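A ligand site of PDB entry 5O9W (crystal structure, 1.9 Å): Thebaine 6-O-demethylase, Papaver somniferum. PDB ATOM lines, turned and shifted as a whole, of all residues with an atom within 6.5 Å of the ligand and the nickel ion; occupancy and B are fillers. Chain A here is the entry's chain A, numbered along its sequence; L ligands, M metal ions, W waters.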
ATOM      1  N   PHE A  90       8.037   7.973  16.009  1.00  0.00           N
ATOM      2  CA  PHE A  90       8.295   9.408  15.987  1.00  0.00           C
ATOM      3  C   PHE A  90       7.784   9.952  17.311  1.00  0.00           C
ATOM      4  O   PHE A  90       6.729   9.500  17.781  1.00  0.00           O
ATOM      5  CB  PHE A  90       7.483  10.142  14.891  1.00  0.00           C
ATOM      6  CG  PHE A  90       8.236  10.344  13.621  1.00  0.00           C
ATOM      7  CD1 PHE A  90       8.360   9.291  12.704  1.00  0.00           C
ATOM      8  CD2 PHE A  90       8.832  11.570  13.324  1.00  0.00           C
ATOM      9  CE1 PHE A  90       9.080   9.457  11.533  1.00  0.00           C
ATOM     10  CE2 PHE A  90       9.532  11.757  12.155  1.00  0.00           C
ATOM     11  CZ  PHE A  90       9.674  10.689  11.257  1.00  0.00           C
ATOM     12  N   ARG A 222      22.104  16.955   7.996  1.00  0.00           N
ATOM     13  CA  ARG A 222      21.525  17.361   6.730  1.00  0.00           C
ATOM     14  C   ARG A 222      20.717  18.625   7.023  1.00  0.00           C
ATOM     15  O   ARG A 222      19.791  18.593   7.800  1.00  0.00           O
ATOM     16  CB  ARG A 222      20.631  16.267   6.182  1.00  0.00           C
ATOM     17  CG  ARG A 222      19.843  16.631   4.955  1.00  0.00           C
ATOM     18  CD  ARG A 222      19.049  15.431   4.437  1.00  0.00           C
ATOM     19  NE  ARG A 222      18.416  15.811   3.201  1.00  0.00           N
ATOM     20  CZ  ARG A 222      18.215  15.011   2.155  1.00  0.00           C
ATOM     21  NH1 ARG A 222      18.515  13.709   2.190  1.00  0.00           N
ATOM     22  NH2 ARG A 222      17.660  15.509   1.062  1.00  0.00           N
ATOM     23  N   ASN A 224      18.271  21.317   5.471  1.00  0.00           N
ATOM     24  CA  ASN A 224      17.306  21.315   4.386  1.00  0.00           C
ATOM     25  C   ASN A 224      16.751  22.713   4.195  1.00  0.00           C
ATOM     26  O   ASN A 224      16.258  23.320   5.171  1.00  0.00           O
ATOM     27  CB  ASN A 224      16.142  20.363   4.691  1.00  0.00           C
ATOM     28  CG  ASN A 224      16.587  18.934   4.900  1.00  0.00           C
ATOM     29  OD1 ASN A 224      17.075  18.268   3.962  1.00  0.00           O
ATOM     30  ND2 ASN A 224      16.393  18.421   6.143  1.00  0.00           N
ATOM     31  N   TYR A 226      13.864  24.562   1.949  1.00  0.00           N
ATOM     32  CA  TYR A 226      12.721  24.292   1.084  1.00  0.00           C
ATOM     33  C   TYR A 226      12.139  25.628   0.619  1.00  0.00           C
ATOM     34  O   TYR A 226      11.435  26.292   1.382  1.00  0.00           O
ATOM     35  CB  TYR A 226      11.661  23.498   1.834  1.00  0.00           C
ATOM     36  CG  TYR A 226      12.106  22.197   2.455  1.00  0.00           C
ATOM     37  CD1 TYR A 226      12.261  21.055   1.693  1.00  0.00           C
ATOM     38  CD2 TYR A 226      12.361  22.096   3.821  1.00  0.00           C
ATOM     39  CE1 TYR A 226      12.646  19.842   2.249  1.00  0.00           C
ATOM     40  CE2 TYR A 226      12.718  20.885   4.389  1.00  0.00           C
ATOM     41  CZ  TYR A 226      12.867  19.771   3.591  1.00  0.00           C
ATOM     42  OH  TYR A 226      13.228  18.572   4.165  1.00  0.00           O
ATOM     43  N   LEU A 238      10.950  16.959   0.240  1.00  0.00           N
ATOM     44  CA  LEU A 238      11.787  15.804   0.426  1.00  0.00           C
ATOM     45  C   LEU A 238      10.926  14.551   0.199  1.00  0.00           C
ATOM     46  O   LEU A 238       9.983  14.293   0.963  1.00  0.00           O
ATOM     47  CB  LEU A 238      12.405  15.832   1.813  1.00  0.00           C
ATOM     48  CG  LEU A 238      13.345  14.666   2.191  1.00  0.00           C
ATOM     49  CD1 LEU A 238      14.517  14.542   1.251  1.00  0.00           C
ATOM     50  CD2 LEU A 238      13.845  14.872   3.620  1.00  0.00           C
ATOM     51  N   HIS A 241      10.503   8.733   2.500  1.00  0.00           N
ATOM     52  CA  HIS A 241      11.596   7.835   2.842  1.00  0.00           C
ATOM     53  C   HIS A 241      11.492   7.424   4.298  1.00  0.00           C
ATOM     54  O   HIS A 241      10.822   8.089   5.092  1.00  0.00           O
ATOM     55  CB  HIS A 241      12.955   8.539   2.620  1.00  0.00           C
ATOM     56  CG  HIS A 241      13.193   9.692   3.552  1.00  0.00           C
ATOM     57  ND1 HIS A 241      12.555  10.910   3.399  1.00  0.00           N
ATOM     58  CD2 HIS A 241      13.931   9.783   4.683  1.00  0.00           C
ATOM     59  CE1 HIS A 241      12.903  11.713   4.400  1.00  0.00           C
ATOM     60  NE2 HIS A 241      13.747  11.050   5.189  1.00  0.00           N
ATOM     61  N   SER A 242      12.159   6.339   4.651  1.00  0.00           N
ATOM     62  CA  SER A 242      12.474   6.073   6.055  1.00  0.00           C
ATOM     63  C   SER A 242      13.958   6.370   6.224  1.00  0.00           C
ATOM     64  O   SER A 242      14.752   6.191   5.271  1.00  0.00           O
ATOM     65  CB  SER A 242      12.094   4.656   6.474  1.00  0.00           C
ATOM     66  OG  SER A 242      12.823   3.667   5.771  1.00  0.00           O
ATOM     67  N   ASP A 243      14.336   6.889   7.392  1.00  0.00           N
ATOM     68  CA  ASP A 243      15.735   7.147   7.676  1.00  0.00           C
ATOM     69  C   ASP A 243      16.430   5.792   7.845  1.00  0.00           C
ATOM     70  O   ASP A 243      15.871   4.847   8.431  1.00  0.00           O
ATOM     71  CB  ASP A 243      15.927   8.033   8.921  1.00  0.00           C
ATOM     72  CG  ASP A 243      15.412   9.437   8.745  1.00  0.00           C
ATOM     73  OD1 ASP A 243      15.196   9.902   7.586  1.00  0.00           O
ATOM     74  OD2 ASP A 243      15.199  10.105   9.784  1.00  0.00           O
ATOM     75  N   THR A 248      17.313   9.746  14.509  1.00  0.00           N
ATOM     76  CA  THR A 248      17.358  11.082  13.921  1.00  0.00           C
ATOM     77  C   THR A 248      16.774  12.077  14.916  1.00  0.00           C
ATOM     78  O   THR A 248      15.725  11.819  15.481  1.00  0.00           O
ATOM     79  CB  THR A 248      16.552  11.131  12.647  1.00  0.00           C
ATOM     80  OG1 THR A 248      17.014  10.114  11.735  1.00  0.00           O
ATOM     81  CG2 THR A 248      16.683  12.494  11.966  1.00  0.00           C
ATOM     82  N   LEU A 250      15.633  15.980  14.805  1.00  0.00           N
ATOM     83  CA  LEU A 250      15.349  17.035  13.830  1.00  0.00           C
ATOM     84  C   LEU A 250      14.970  18.332  14.544  1.00  0.00           C
ATOM     85  O   LEU A 250      14.171  18.304  15.502  1.00  0.00           O
ATOM     86  CB  LEU A 250      14.166  16.607  12.960  1.00  0.00           C
ATOM     87  CG  LEU A 250      13.683  17.633  11.915  1.00  0.00           C
ATOM     88  CD1 LEU A 250      14.417  17.439  10.613  1.00  0.00           C
ATOM     89  CD2 LEU A 250      12.197  17.471  11.692  1.00  0.00           C
ATOM     90  N   GLN A 252      13.268  21.928  13.473  1.00  0.00           N
ATOM     91  CA  GLN A 252      12.645  22.795  12.503  1.00  0.00           C
ATOM     92  C   GLN A 252      13.114  24.196  12.822  1.00  0.00           C
ATOM     93  O   GLN A 252      12.915  24.713  13.971  1.00  0.00           O
ATOM     94  CB  GLN A 252      11.130  22.662  12.535  1.00  0.00           C
ATOM     95  CG  GLN A 252      10.420  23.437  11.437  1.00  0.00           C
ATOM     96  CD  GLN A 252       8.939  23.152  11.432  1.00  0.00           C
ATOM     97  OE1 GLN A 252       8.498  22.167  10.899  1.00  0.00           O
ATOM     98  NE2 GLN A 252       8.165  24.028  12.043  1.00  0.00           N
ATOM     99  N   GLY A 258       5.641  21.429   7.542  1.00  0.00           N
ATOM    100  CA  GLY A 258       5.975  20.648   6.365  1.00  0.00           C
ATOM    101  C   GLY A 258       6.289  19.184   6.530  1.00  0.00           C
ATOM    102  O   GLY A 258       6.152  18.419   5.560  1.00  0.00           O
ATOM    103  N   LEU A 259       6.762  18.812   7.719  1.00  0.00           N
ATOM    104  CA  LEU A 259       7.017  17.413   8.006  1.00  0.00           C
ATOM    105  C   LEU A 259       5.694  16.622   8.095  1.00  0.00           C
ATOM    106  O   LEU A 259       4.777  17.026   8.833  1.00  0.00           O
ATOM    107  CB  LEU A 259       7.806  17.255   9.292  1.00  0.00           C
ATOM    108  CG  LEU A 259       8.041  15.829   9.797  1.00  0.00           C
ATOM    109  CD1 LEU A 259       8.879  15.049   8.788  1.00  0.00           C
ATOM    110  CD2 LEU A 259       8.707  15.871  11.134  1.00  0.00           C
ATOM    111  N   GLN A 260       5.625  15.511   7.380  1.00  0.00           N
ATOM    112  CA  GLN A 260       4.505  14.568   7.493  1.00  0.00           C
ATOM    113  C   GLN A 260       4.999  13.148   7.615  1.00  0.00           C
ATOM    114  O   GLN A 260       6.015  12.813   7.026  1.00  0.00           O
ATOM    115  CB  GLN A 260       3.581  14.673   6.278  1.00  0.00           C
ATOM    116  CG  GLN A 260       3.032  16.083   6.028  1.00  0.00           C
ATOM    117  CD  GLN A 260       2.138  16.170   4.802  1.00  0.00           C
ATOM    118  OE1 GLN A 260       2.123  15.279   3.952  1.00  0.00           O
ATOM    119  NE2 GLN A 260       1.432  17.306   4.682  1.00  0.00           N
ATOM    120  N   ASN A 280      13.102  10.382  15.560  1.00  0.00           N
ATOM    121  CA  ASN A 280      12.526   9.180  14.960  1.00  0.00           C
ATOM    122  C   ASN A 280      13.528   8.038  14.842  1.00  0.00           C
ATOM    123  O   ASN A 280      14.748   8.260  14.716  1.00  0.00           O
ATOM    124  CB  ASN A 280      11.876   9.440  13.585  1.00  0.00           C
ATOM    125  CG  ASN A 280      12.872   9.842  12.489  1.00  0.00           C
ATOM    126  OD1 ASN A 280      13.382  10.965  12.493  1.00  0.00           O
ATOM    127  ND2 ASN A 280      13.119   8.922  11.492  1.00  0.00           N
ATOM    128  N   HIS A 298       8.365   9.046   6.028  1.00  0.00           N
ATOM    129  CA  HIS A 298       8.026  10.451   6.204  1.00  0.00           C
ATOM    130  C   HIS A 298       8.497  11.278   4.998  1.00  0.00           C
ATOM    131  O   HIS A 298       9.295  10.836   4.172  1.00  0.00           O
ATOM    132  CB  HIS A 298       8.589  10.986   7.523  1.00  0.00           C
ATOM    133  CG  HIS A 298      10.061  10.782   7.670  1.00  0.00           C
ATOM    134  ND1 HIS A 298      10.619   9.555   7.972  1.00  0.00           N
ATOM    135  CD2 HIS A 298      11.093  11.634   7.509  1.00  0.00           C
ATOM    136  CE1 HIS A 298      11.928   9.675   8.000  1.00  0.00           C
ATOM    137  NE2 HIS A 298      12.255  10.929   7.728  1.00  0.00           N
ATOM    138  N   ARG A 299       7.926  12.450   4.871  1.00  0.00           N
ATOM    139  CA  ARG A 299       8.234  13.382   3.759  1.00  0.00           C
ATOM    140  C   ARG A 299       8.150  14.813   4.232  1.00  0.00           C
ATOM    141  O   ARG A 299       7.650  15.067   5.325  1.00  0.00           O
ATOM    142  CB  ARG A 299       7.254  13.142   2.603  1.00  0.00           C
ATOM    143  CG  ARG A 299       5.849  13.620   2.883  1.00  0.00           C
ATOM    144  CD  ARG A 299       4.876  13.188   1.796  1.00  0.00           C
ATOM    145  NE  ARG A 299       3.564  13.753   2.038  1.00  0.00           N
ATOM    146  CZ  ARG A 299       2.539  13.733   1.171  1.00  0.00           C
ATOM    147  NH1 ARG A 299       2.659  13.161  -0.007  1.00  0.00           N
ATOM    148  NH2 ARG A 299       1.377  14.283   1.527  1.00  0.00           N
ATOM    149  N   ALA A 300       8.594  15.745   3.400  1.00  0.00           N
ATOM    150  CA  ALA A 300       8.432  17.152   3.692  1.00  0.00           C
ATOM    151  C   ALA A 300       7.773  17.790   2.504  1.00  0.00           C
ATOM    152  O   ALA A 300       8.207  17.648   1.354  1.00  0.00           O
ATOM    153  CB  ALA A 300       9.765  17.814   3.983  1.00  0.00           C
ATOM    154  N   ARG A 308      10.828  26.966   4.155  1.00  0.00           N
ATOM    155  CA  ARG A 308      10.928  26.176   5.382  1.00  0.00           C
ATOM    156  C   ARG A 308      12.382  25.700   5.480  1.00  0.00           C
ATOM    157  O   ARG A 308      12.976  25.328   4.476  1.00  0.00           O
ATOM    158  CB  ARG A 308       9.999  24.974   5.321  1.00  0.00           C
ATOM    159  CG  ARG A 308       9.981  24.122   6.581  1.00  0.00           C
ATOM    160  CD  ARG A 308       8.860  23.109   6.609  1.00  0.00           C
ATOM    161  NE  ARG A 308       9.076  22.263   7.762  1.00  0.00           N
ATOM    162  CZ  ARG A 308       9.789  21.129   7.766  1.00  0.00           C
ATOM    163  NH1 ARG A 308       9.983  20.532   8.924  1.00  0.00           N
ATOM    164  NH2 ARG A 308      10.265  20.572   6.655  1.00  0.00           N
ATOM    165  N   LEU A 309      12.954  25.767   6.673  1.00  0.00           N
ATOM    166  CA  LEU A 309      14.281  25.221   6.950  1.00  0.00           C
ATOM    167  C   LEU A 309      14.218  24.162   8.064  1.00  0.00           C
ATOM    168  O   LEU A 309      13.444  24.291   9.008  1.00  0.00           O
ATOM    169  CB  LEU A 309      15.261  26.331   7.348  1.00  0.00           C
ATOM    170  CG  LEU A 309      15.699  27.274   6.216  1.00  0.00           C
ATOM    171  CD1 LEU A 309      14.668  28.353   5.968  1.00  0.00           C
ATOM    172  CD2 LEU A 309      17.056  27.900   6.518  1.00  0.00           C
ATOM    173  N   SER A 310      15.095  23.162   7.983  1.00  0.00           N
ATOM    174  CA  SER A 310      15.228  22.168   9.023  1.00  0.00           C
ATOM    175  C   SER A 310      16.666  21.636   9.032  1.00  0.00           C
ATOM    176  O   SER A 310      17.390  21.785   8.032  1.00  0.00           O
ATOM    177  CB  SER A 310      14.229  21.024   8.821  1.00  0.00           C
ATOM    178  OG  SER A 310      14.523  20.207   7.701  1.00  0.00           O
ATOM    179  N   ILE A 311      17.062  21.063  10.173  1.00  0.00           N
ATOM    180  CA  ILE A 311      18.342  20.362  10.268  1.00  0.00           C
ATOM    181  C   ILE A 311      18.088  19.025  10.973  1.00  0.00           C
ATOM    182  O   ILE A 311      17.593  18.969  12.094  1.00  0.00           O
ATOM    183  CB  ILE A 311      19.480  21.188  10.899  1.00  0.00           C
ATOM    184  CG1 ILE A 311      20.768  20.337  10.981  1.00  0.00           C
ATOM    185  CG2 ILE A 311      19.062  21.760  12.265  1.00  0.00           C
ATOM    186  CD1 ILE A 311      21.979  21.036  11.526  1.00  0.00           C
ATOM    187  N   ALA A 312      18.430  17.951  10.274  1.00  0.00           N
ATOM    188  CA  ALA A 312      18.312  16.603  10.781  1.00  0.00           C
ATOM    189  C   ALA A 312      19.725  16.136  11.193  1.00  0.00           C
ATOM    190  O   ALA A 312      20.658  16.227  10.392  1.00  0.00           O
ATOM    191  CB  ALA A 312      17.764  15.713   9.697  1.00  0.00           C
ATOM    192  N   PHE A 314      21.656  12.750  12.331  1.00  0.00           N
ATOM    193  CA  PHE A 314      21.518  11.313  12.285  1.00  0.00           C
ATOM    194  C   PHE A 314      22.565  10.662  13.157  1.00  0.00           C
ATOM    195  O   PHE A 314      23.736  11.027  13.094  1.00  0.00           O
ATOM    196  CB  PHE A 314      21.709  10.824  10.851  1.00  0.00           C
ATOM    197  CG  PHE A 314      20.813  11.478   9.884  1.00  0.00           C
ATOM    198  CD1 PHE A 314      19.480  11.102   9.780  1.00  0.00           C
ATOM    199  CD2 PHE A 314      21.281  12.502   9.067  1.00  0.00           C
ATOM    200  CE1 PHE A 314      18.623  11.734   8.900  1.00  0.00           C
ATOM    201  CE2 PHE A 314      20.428  13.129   8.180  1.00  0.00           C
ATOM    202  CZ  PHE A 314      19.095  12.758   8.111  1.00  0.00           C
HETATM  203  C1  LIG L   1      15.576  14.135   6.659  1.00  0.00           C
HETATM  204  O1  LIG L   1      15.764  12.890   6.638  1.00  0.00           O
HETATM  205  O2  LIG L   1      16.492  14.948   6.516  1.00  0.00           O
HETATM  206  C2  LIG L   1      14.194  14.617   6.842  1.00  0.00           C
HETATM  207  O3  LIG L   1      13.288  13.783   6.834  1.00  0.00           O
HETATM  208  C3  LIG L   1      13.898  16.059   7.068  1.00  0.00           C
HETATM  209  C4  LIG L   1      12.411  16.317   7.323  1.00  0.00           C
HETATM  210  C5  LIG L   1      12.083  17.789   7.460  1.00  0.00           C
HETATM  211  O4  LIG L   1      12.737  18.622   6.763  1.00  0.00           O
HETATM  212  O5  LIG L   1      11.186  18.102   8.283  1.00  0.00           O
HETATM  213 NI    NI M   1      14.118  11.759   7.170  1.00  0.00          NI
HETATM  214  O   HOH W   1      14.457  12.439   9.128  1.00  0.00           O
HETATM  215  O   HOH W   2      17.372  12.116   4.302  1.00  0.00           O
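O1 of the ligand is bound to the nickel ion (2.1 Å). The nickel ion is bound by water W1, at 2.1 Å. The nickel ion is bound by a ring nitrogen (NE2) of His 298 (2.1 Å). NE2 of His 241 is bound to the nickel ion, 2.1 Å away. The nickel ion is bound by OD1 of Asp 243. The nickel ion is bound by an oxygen (O3) of the ligand, at 2.2 Å.
The side-chain hydroxyl (OH) of Tyr 226 lies within hydrogen-bond range of an oxygen (O4) of the ligand. The guanidinium group (NH1) of Arg 308 is in salt-bridge range of an oxygen (O5) of the ligand, 2.8 Å away. The side-chain amide nitrogen (ND2) of Asn 224 lies within hydrogen-bond range of an oxygen (O2) of the ligand (3.5 Å). NE of Arg 222 is in salt-bridge range of O2 of the ligand. The side-chain hydroxyl of Ser 310 sits at hydrogen-bond distance from an oxygen (O4) of the ligand, 2.6 Å away.
Merely in contact with the ligand: Leu 238, Leu 250, Leu 259, Ala 312 and Phe 314. Hydrophobic or aromatic side chains that line the ligand: Tyr 226, Leu 238, His 241, Leu 250, Leu 259, His 298, Ala 312 and Phe 314. Within 4 Å of the ligand: Arg 222, Asn 224, Tyr 226, Leu 238, His 241, Asp 243, Leu 250, Leu 259, His 298, Arg 308, Ser 310, Ala 312 and Phe 314. The nearest printed residue that does not touch the ligand is Ala 300 (4.1 Å).
Within 4 Å of the nickel ion: His 241, Asp 243 and His 298. The nearest printed residue that does not touch the nickel ion is Leu 238 (4.7 Å).
OE1 of Gln 252 sits at hydrogen-bond distance from NH1 of Arg 308. The backbone carbonyl oxygen of Ser 310 is in hydrogen-bond range of the backbone NH of Asn 224 (2.7 Å). ND2 of Asn 280 is in hydrogen-bond range of OD2 of Asp 243, at 2.9 Å. The backbone carbonyl oxygen (O) of Arg 308 sits at hydrogen-bond distance from the backbone NH (N) of Tyr 226. OG1 of Thr 248 sits at hydrogen-bond distance from OD2 of Asp 243 (2.7 Å). N of Arg 222 is in hydrogen-bond range of O of Ala 312, 2.9 Å away. The backbone carbonyl oxygen (O) of Ala 300 lies within hydrogen-bond range of the backbone NH (N) of Leu 238 (3.0 Å). The guanidinium group (NE) of Arg 222 lies within hydrogen-bond range of the side-chain amide oxygen (OD1) of Asn 224 (2.9 Å).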
